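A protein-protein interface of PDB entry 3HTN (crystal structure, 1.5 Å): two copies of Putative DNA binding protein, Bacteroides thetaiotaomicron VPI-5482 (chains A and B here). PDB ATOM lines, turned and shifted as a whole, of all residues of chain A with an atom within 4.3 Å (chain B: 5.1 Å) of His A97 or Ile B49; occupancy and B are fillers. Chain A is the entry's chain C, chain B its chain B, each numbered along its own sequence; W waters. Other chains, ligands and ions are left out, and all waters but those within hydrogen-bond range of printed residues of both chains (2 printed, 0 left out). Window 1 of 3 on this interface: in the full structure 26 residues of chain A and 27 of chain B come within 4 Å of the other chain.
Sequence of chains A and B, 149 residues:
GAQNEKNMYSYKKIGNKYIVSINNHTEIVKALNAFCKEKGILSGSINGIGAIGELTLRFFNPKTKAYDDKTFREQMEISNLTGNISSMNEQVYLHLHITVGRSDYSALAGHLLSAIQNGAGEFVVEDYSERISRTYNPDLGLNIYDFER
The backbone carbonyl oxygen of Ile B78 is in hydrogen-bond range of a ring nitrogen (ND1) of His A97, 2.7 Å away. The side-chain carboxylate of Glu B122 is in hydrogen-bond range of a ring nitrogen (ND1) of His A95 (2.8 Å). The side-chain amide oxygen (OD1) of Asn B80 lies within hydrogen-bond range of the side-chain hydroxyl (OG1) of Thr A82 (2.9 Å). The side-chain carboxylate of Glu B122 is in hydrogen-bond range of the side-chain amide nitrogen of Asn A84.
The backbone carbonyl oxygen of Ile B49 is in hydrogen-bond range of the backbone NH of Glu B122 (2.9 Å). N of His A97 is in hydrogen-bond range of O of Thr A82 (2.8 Å). N of Asn A84 sits at hydrogen-bond distance from O of His A95 (2.9 Å). NE2 of His A97 sits at hydrogen-bond distance from NE2 of His A95. The backbone NH (N) of Ile A98 sits at hydrogen-bond distance from the backbone carbonyl oxygen (O) of Gly A110, 2.9 Å away. The backbone NH (N) of Ile B78 sits at hydrogen-bond distance from the backbone carbonyl oxygen (O) of Gly B50, 2.7 Å away.
Thr A82 touches Ile B49. Thr A82 touches Ser B79. CD1 of Ile B49 touches O of His A95, at 3.6 Å. His A97 touches Ile B49. His A97 touches Gly B50 (CE1 to O, 3.7 Å). Glu B77 touches His A97. His A97 touches Ser B79 (CB to O, 3.7 Å). Ser B79 touches Ile A98 (CB to O, 3.4 Å).
Of the printed residues of chain B, His A97 touches Ile B49 (3.7 Å), Gly B50 (3.7 Å), Glu B77 (3.2 Å), Ile B78 (2.7 Å) and Ser B79 (3.7 Å). His A111 touches none of the printed residues of chain B. Leu A112 touches none of the printed residues of chain B. Of the printed residues of chain A, Ile B49 touches Thr A82 (3.7 Å), His A95 (3.6 Å) and His A97 (3.7 Å). Of the printed residues of chain A, Gly B50 touches His A97. Printed residues of chain A within 4 Å of Ile B78: His A97. The nearest printed residue of chain B that does not touch His A97 is Ala B51 (5.4 Å). The nearest printed residue of chain A that does not touch Ile B49 is Asn A84 (4.04 Å). The nearest printed residue of chain B that does not touch Thr A82 is Gly B48 (4.4 Å).
Hydrophobic or aromatic side chains of chain B within 4 Å of the printed part of chain A: Ile B49. Along chain B the printed residues that touch a printed residue of chain A span positions 49 to 122. Of the 10 printed residues of chain A, 5 touch a printed residue of chain B. Hydrophobic or aromatic side chains of chain A within 4 Å of the printed part of chain B: His A95 and His A97. Among the printed residues, 12 pairs touch across the chains.
No position is printed for both chains.
Water W1 lies within hydrogen-bond range of the side-chain carboxylate (OE1) of Glu B77 and a ring nitrogen (NE2) of His A97. Water W2 lies within hydrogen-bond range of O of Glu B122 and ND2 of Asn A84.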
ATOM      1  N   LEU A  81      32.756  13.158   6.592  1.00  0.00           N
ATOM      2  CA  LEU A  81      31.331  12.928   6.874  1.00  0.00           C
ATOM      3  C   LEU A  81      31.234  13.127   8.377  1.00  0.00           C
ATOM      4  O   LEU A  81      32.014  12.540   9.125  1.00  0.00           O
ATOM      5  CB  LEU A  81      30.911  11.550   6.465  1.00  0.00           C
ATOM      6  CG  LEU A  81      29.433  11.168   6.671  1.00  0.00           C
ATOM      7  CD1 LEU A  81      29.060  10.100   5.666  1.00  0.00           C
ATOM      8  CD2 LEU A  81      29.189  10.687   8.115  1.00  0.00           C
ATOM      9  N   THR A  82      30.354  14.052   8.806  1.00  0.00           N
ATOM     10  CA  THR A  82      30.129  14.451  10.227  1.00  0.00           C
ATOM     11  C   THR A  82      28.641  14.303  10.569  1.00  0.00           C
ATOM     12  O   THR A  82      27.798  14.879   9.887  1.00  0.00           O
ATOM     13  CB  THR A  82      30.513  15.949  10.513  1.00  0.00           C
ATOM     14  OG1 THR A  82      31.864  16.226  10.108  1.00  0.00           O
ATOM     15  CG2 THR A  82      30.360  16.309  12.031  1.00  0.00           C
ATOM     16  N   ASN A  84      25.420  12.825  13.649  1.00  0.00           N
ATOM     17  CA  ASN A  84      25.012  12.379  14.969  1.00  0.00           C
ATOM     18  C   ASN A  84      23.862  11.407  14.888  1.00  0.00           C
ATOM     19  O   ASN A  84      23.177  11.289  13.853  1.00  0.00           O
ATOM     20  CB  ASN A  84      24.741  13.603  15.859  1.00  0.00           C
ATOM     21  CG  ASN A  84      23.711  14.535  15.311  1.00  0.00           C
ATOM     22  OD1 ASN A  84      22.595  14.108  15.023  1.00  0.00           O
ATOM     23  ND2 ASN A  84      24.046  15.842  15.195  1.00  0.00           N
ATOM     24  N   HIS A  95      21.492  12.299  11.541  1.00  0.00           N
ATOM     25  CA  HIS A  95      21.628  13.623  10.949  1.00  0.00           C
ATOM     26  C   HIS A  95      23.076  13.710  10.496  1.00  0.00           C
ATOM     27  O   HIS A  95      23.983  13.833  11.317  1.00  0.00           O
ATOM     28  CB  HIS A  95      21.278  14.708  11.963  1.00  0.00           C
ATOM     29  CG  HIS A  95      21.224  16.079  11.387  1.00  0.00           C
ATOM     30  ND1 HIS A  95      21.240  17.204  12.181  1.00  0.00           N
ATOM     31  CD2 HIS A  95      21.196  16.517  10.106  1.00  0.00           C
ATOM     32  CE1 HIS A  95      21.197  18.280  11.411  1.00  0.00           C
ATOM     33  NE2 HIS A  95      21.130  17.892  10.149  1.00  0.00           N
ATOM     34  N   LEU A  96      23.284  13.638   9.180  1.00  0.00           N
ATOM     35  CA  LEU A  96      24.614  13.522   8.600  1.00  0.00           C
ATOM     36  C   LEU A  96      24.858  14.633   7.584  1.00  0.00           C
ATOM     37  O   LEU A  96      24.017  14.887   6.715  1.00  0.00           O
ATOM     38  CB  LEU A  96      24.770  12.199   7.877  1.00  0.00           C
ATOM     39  CG  LEU A  96      24.370  10.929   8.654  1.00  0.00           C
ATOM     40  CD1 LEU A  96      24.597   9.736   7.737  1.00  0.00           C
ATOM     41  CD2 LEU A  96      25.141  10.779   9.941  1.00  0.00           C
ATOM     42  N   HIS A  97      25.993  15.286   7.720  1.00  0.00           N
ATOM     43  CA  HIS A  97      26.453  16.253   6.722  1.00  0.00           C
ATOM     44  C   HIS A  97      27.750  15.718   6.126  1.00  0.00           C
ATOM     45  O   HIS A  97      28.388  14.791   6.661  1.00  0.00           O
ATOM     46  CB  HIS A  97      26.661  17.638   7.310  1.00  0.00           C
ATOM     47  CG  HIS A  97      25.384  18.378   7.610  1.00  0.00           C
ATOM     48  ND1 HIS A  97      25.385  19.732   7.867  1.00  0.00           N
ATOM     49  CD2 HIS A  97      24.096  17.979   7.716  1.00  0.00           C
ATOM     50  CE1 HIS A  97      24.148  20.137   8.102  1.00  0.00           C
ATOM     51  NE2 HIS A  97      23.340  19.100   8.001  1.00  0.00           N
ATOM     52  N   ILE A  98      28.153  16.319   5.021  1.00  0.00           N
ATOM     53  CA  ILE A  98      29.275  15.792   4.288  1.00  0.00           C
ATOM     54  C   ILE A  98      29.968  16.866   3.490  1.00  0.00           C
ATOM     55  O   ILE A  98      29.358  17.852   3.066  1.00  0.00           O
ATOM     56  CB  ILE A  98      28.824  14.612   3.359  1.00  0.00           C
ATOM     57  CG1 ILE A  98      29.987  13.716   2.892  1.00  0.00           C
ATOM     58  CG2 ILE A  98      28.012  15.148   2.146  1.00  0.00           C
ATOM     59  CD1 ILE A  98      29.480  12.458   2.133  1.00  0.00           C
ATOM     60  N   GLY A 110      27.181  19.738   2.208  1.00  0.00           N
ATOM     61  CA  GLY A 110      25.822  19.917   2.629  1.00  0.00           C
ATOM     62  C   GLY A 110      25.263  18.791   3.462  1.00  0.00           C
ATOM     63  O   GLY A 110      25.992  17.970   3.991  1.00  0.00           O
ATOM     64  N   HIS A 111      23.938  18.783   3.561  1.00  0.00           N
ATOM     65  CA  HIS A 111      23.185  17.737   4.243  1.00  0.00           C
ATOM     66  C   HIS A 111      23.121  16.510   3.350  1.00  0.00           C
ATOM     67  O   HIS A 111      22.597  16.563   2.227  1.00  0.00           O
ATOM     68  CB  HIS A 111      21.788  18.294   4.569  1.00  0.00           C
ATOM     69  CG  HIS A 111      20.810  17.313   5.118  1.00  0.00           C
ATOM     70  ND1 HIS A 111      21.149  16.230   5.904  1.00  0.00           N
ATOM     71  CD2 HIS A 111      19.460  17.311   5.050  1.00  0.00           C
ATOM     72  CE1 HIS A 111      20.041  15.600   6.274  1.00  0.00           C
ATOM     73  NE2 HIS A 111      19.015  16.209   5.734  1.00  0.00           N
ATOM     74  N   LEU A 112      23.628  15.395   3.879  1.00  0.00           N
ATOM     75  CA  LEU A 112      23.724  14.163   3.157  1.00  0.00           C
ATOM     76  C   LEU A 112      22.429  13.373   3.212  1.00  0.00           C
ATOM     77  O   LEU A 112      21.958  13.014   4.277  1.00  0.00           O
ATOM     78  CB  LEU A 112      24.845  13.318   3.768  1.00  0.00           C
ATOM     79  CG  LEU A 112      25.019  11.896   3.240  1.00  0.00           C
ATOM     80  CD1 LEU A 112      25.433  11.926   1.764  1.00  0.00           C
ATOM     81  CD2 LEU A 112      26.012  11.106   4.097  1.00  0.00           C
ATOM     82  N   ASN B  47      32.985  20.035  17.821  1.00  0.00           N
ATOM     83  CA  ASN B  47      32.679  19.539  16.479  1.00  0.00           C
ATOM     84  C   ASN B  47      31.193  19.568  16.272  1.00  0.00           C
ATOM     85  O   ASN B  47      30.455  19.191  17.150  1.00  0.00           O
ATOM     86  CB  ASN B  47      33.179  18.111  16.319  1.00  0.00           C
ATOM     87  CG  ASN B  47      34.646  18.037  16.330  1.00  0.00           C
ATOM     88  OD1 ASN B  47      35.273  18.276  15.298  1.00  0.00           O
ATOM     89  ND2 ASN B  47      35.245  17.740  17.494  1.00  0.00           N
ATOM     90  N   GLY B  48      30.734  19.982  15.105  1.00  0.00           N
ATOM     91  CA  GLY B  48      29.307  19.827  14.831  1.00  0.00           C
ATOM     92  C   GLY B  48      28.844  20.315  13.505  1.00  0.00           C
ATOM     93  O   GLY B  48      29.642  20.635  12.635  1.00  0.00           O
ATOM     94  N   ILE B  49      27.527  20.415  13.384  1.00  0.00           N
ATOM     95  CA  ILE B  49      26.844  20.696  12.127  1.00  0.00           C
ATOM     96  C   ILE B  49      25.617  21.569  12.432  1.00  0.00           C
ATOM     97  O   ILE B  49      25.193  21.700  13.599  1.00  0.00           O
ATOM     98  CB  ILE B  49      26.411  19.385  11.423  1.00  0.00           C
ATOM     99  CG1 ILE B  49      25.489  18.514  12.298  1.00  0.00           C
ATOM    100  CG2 ILE B  49      27.614  18.535  11.026  1.00  0.00           C
ATOM    101  CD1 ILE B  49      24.853  17.326  11.529  1.00  0.00           C
ATOM    102  N   GLY B  50      25.014  22.133  11.400  1.00  0.00           N
ATOM    103  CA  GLY B  50      23.842  22.985  11.553  1.00  0.00           C
ATOM    104  C   GLY B  50      23.661  23.819  10.319  1.00  0.00           C
ATOM    105  O   GLY B  50      24.330  23.577   9.341  1.00  0.00           O
ATOM    106  N   ALA B  51      22.751  24.779  10.381  1.00  0.00           N
ATOM    107  CA  ALA B  51      22.431  25.641   9.269  1.00  0.00           C
ATOM    108  C   ALA B  51      22.490  27.070   9.744  1.00  0.00           C
ATOM    109  O   ALA B  51      22.152  27.377  10.901  1.00  0.00           O
ATOM    110  CB  ALA B  51      21.022  25.327   8.727  1.00  0.00           C
ATOM    111  N   GLU B  77      24.601  25.522   4.808  1.00  0.00           N
ATOM    112  CA  GLU B  77      24.686  24.382   5.717  1.00  0.00           C
ATOM    113  C   GLU B  77      26.101  24.238   6.232  1.00  0.00           C
ATOM    114  O   GLU B  77      27.059  24.232   5.432  1.00  0.00           O
ATOM    115  CB  GLU B  77      24.268  23.086   5.031  1.00  0.00           C
ATOM    116  CG  GLU B  77      22.762  23.018   4.751  1.00  0.00           C
ATOM    117  CD  GLU B  77      21.903  22.850   6.005  1.00  0.00           C
ATOM    118  OE1 GLU B  77      22.431  22.680   7.133  1.00  0.00           O
ATOM    119  OE2 GLU B  77      20.645  22.935   5.867  1.00  0.00           O
ATOM    120  N   ILE B  78      26.270  24.102   7.533  1.00  0.00           N
ATOM    121  CA  ILE B  78      27.585  23.862   8.094  1.00  0.00           C
ATOM    122  C   ILE B  78      27.872  22.377   7.912  1.00  0.00           C
ATOM    123  O   ILE B  78      27.262  21.539   8.584  1.00  0.00           O
ATOM    124  CB  ILE B  78      27.665  24.162   9.583  1.00  0.00           C
ATOM    125  CG1 ILE B  78      27.349  25.636   9.871  1.00  0.00           C
ATOM    126  CG2 ILE B  78      29.072  23.790  10.113  1.00  0.00           C
ATOM    127  CD1 ILE B  78      27.229  25.949  11.407  1.00  0.00           C
ATOM    128  N   SER B  79      28.754  22.023   6.989  1.00  0.00           N
ATOM    129  CA  SER B  79      29.065  20.614   6.796  1.00  0.00           C
ATOM    130  C   SER B  79      30.004  20.090   7.867  1.00  0.00           C
ATOM    131  O   SER B  79      29.964  18.914   8.216  1.00  0.00           O
ATOM    132  CB  SER B  79      29.627  20.350   5.386  1.00  0.00           C
ATOM    133  OG  SER B  79      30.869  20.982   5.153  1.00  0.00           O
ATOM    134  N   ASN B  80      30.841  20.956   8.402  1.00  0.00           N
ATOM    135  CA  ASN B  80      31.667  20.644   9.513  1.00  0.00           C
ATOM    136  C   ASN B  80      32.147  21.915  10.187  1.00  0.00           C
ATOM    137  O   ASN B  80      32.603  22.843   9.521  1.00  0.00           O
ATOM    138  CB  ASN B  80      32.861  19.821   9.069  1.00  0.00           C
ATOM    139  CG  ASN B  80      33.764  19.505  10.183  1.00  0.00           C
ATOM    140  OD1 ASN B  80      33.604  18.469  10.847  1.00  0.00           O
ATOM    141  ND2 ASN B  80      34.740  20.373  10.427  1.00  0.00           N
ATOM    142  N   ALA B 120      19.056  24.360  12.746  1.00  0.00           N
ATOM    143  CA  ALA B 120      19.610  23.630  13.877  1.00  0.00           C
ATOM    144  C   ALA B 120      21.074  23.983  14.074  1.00  0.00           C
ATOM    145  O   ALA B 120      21.747  24.546  13.202  1.00  0.00           O
ATOM    146  CB  ALA B 120      19.475  22.112  13.669  1.00  0.00           C
ATOM    147  N   GLY B 121      21.592  23.639  15.240  1.00  0.00           N
ATOM    148  CA  GLY B 121      22.985  23.867  15.626  1.00  0.00           C
ATOM    149  C   GLY B 121      23.298  22.813  16.642  1.00  0.00           C
ATOM    150  O   GLY B 121      22.900  22.914  17.795  1.00  0.00           O
ATOM    151  N   GLU B 122      24.010  21.792  16.196  1.00  0.00           N
ATOM    152  CA  GLU B 122      24.207  20.555  16.947  1.00  0.00           C
ATOM    153  C   GLU B 122      25.684  20.313  17.082  1.00  0.00           C
ATOM    154  O   GLU B 122      26.350  19.924  16.121  1.00  0.00           O
ATOM    155  CB  GLU B 122      23.520  19.415  16.190  1.00  0.00           C
ATOM    156  CG  GLU B 122      22.005  19.629  16.127  1.00  0.00           C
ATOM    157  CD  GLU B 122      21.242  18.672  15.251  1.00  0.00           C
ATOM    158  OE1 GLU B 122      21.818  17.635  14.836  1.00  0.00           O
ATOM    159  OE2 GLU B 122      20.040  18.954  15.005  1.00  0.00           O
ATOM    160  N   PHE B 123      26.209  20.533  18.283  1.00  0.00           N
ATOM    161  CA  PHE B 123      27.643  20.475  18.541  1.00  0.00           C
ATOM    162  C   PHE B 123      28.011  19.578  19.700  1.00  0.00           C
ATOM    163  O   PHE B 123      27.303  19.537  20.691  1.00  0.00           O
ATOM    164  CB  PHE B 123      28.189  21.899  18.786  1.00  0.00           C
ATOM    165  CG  PHE B 123      27.904  22.838  17.660  1.00  0.00           C
ATOM    166  CD1 PHE B 123      28.716  22.855  16.550  1.00  0.00           C
ATOM    167  CD2 PHE B 123      26.760  23.606  17.638  1.00  0.00           C
ATOM    168  CE1 PHE B 123      28.419  23.649  15.481  1.00  0.00           C
ATOM    169  CE2 PHE B 123      26.475  24.418  16.567  1.00  0.00           C
ATOM    170  CZ  PHE B 123      27.297  24.440  15.496  1.00  0.00           C
HETATM  171  O   HOH W   1      21.433  21.391   9.444  1.00  0.00           O
HETATM  172  O   HOH W   2      26.578  17.058  16.131  1.00  0.00           O
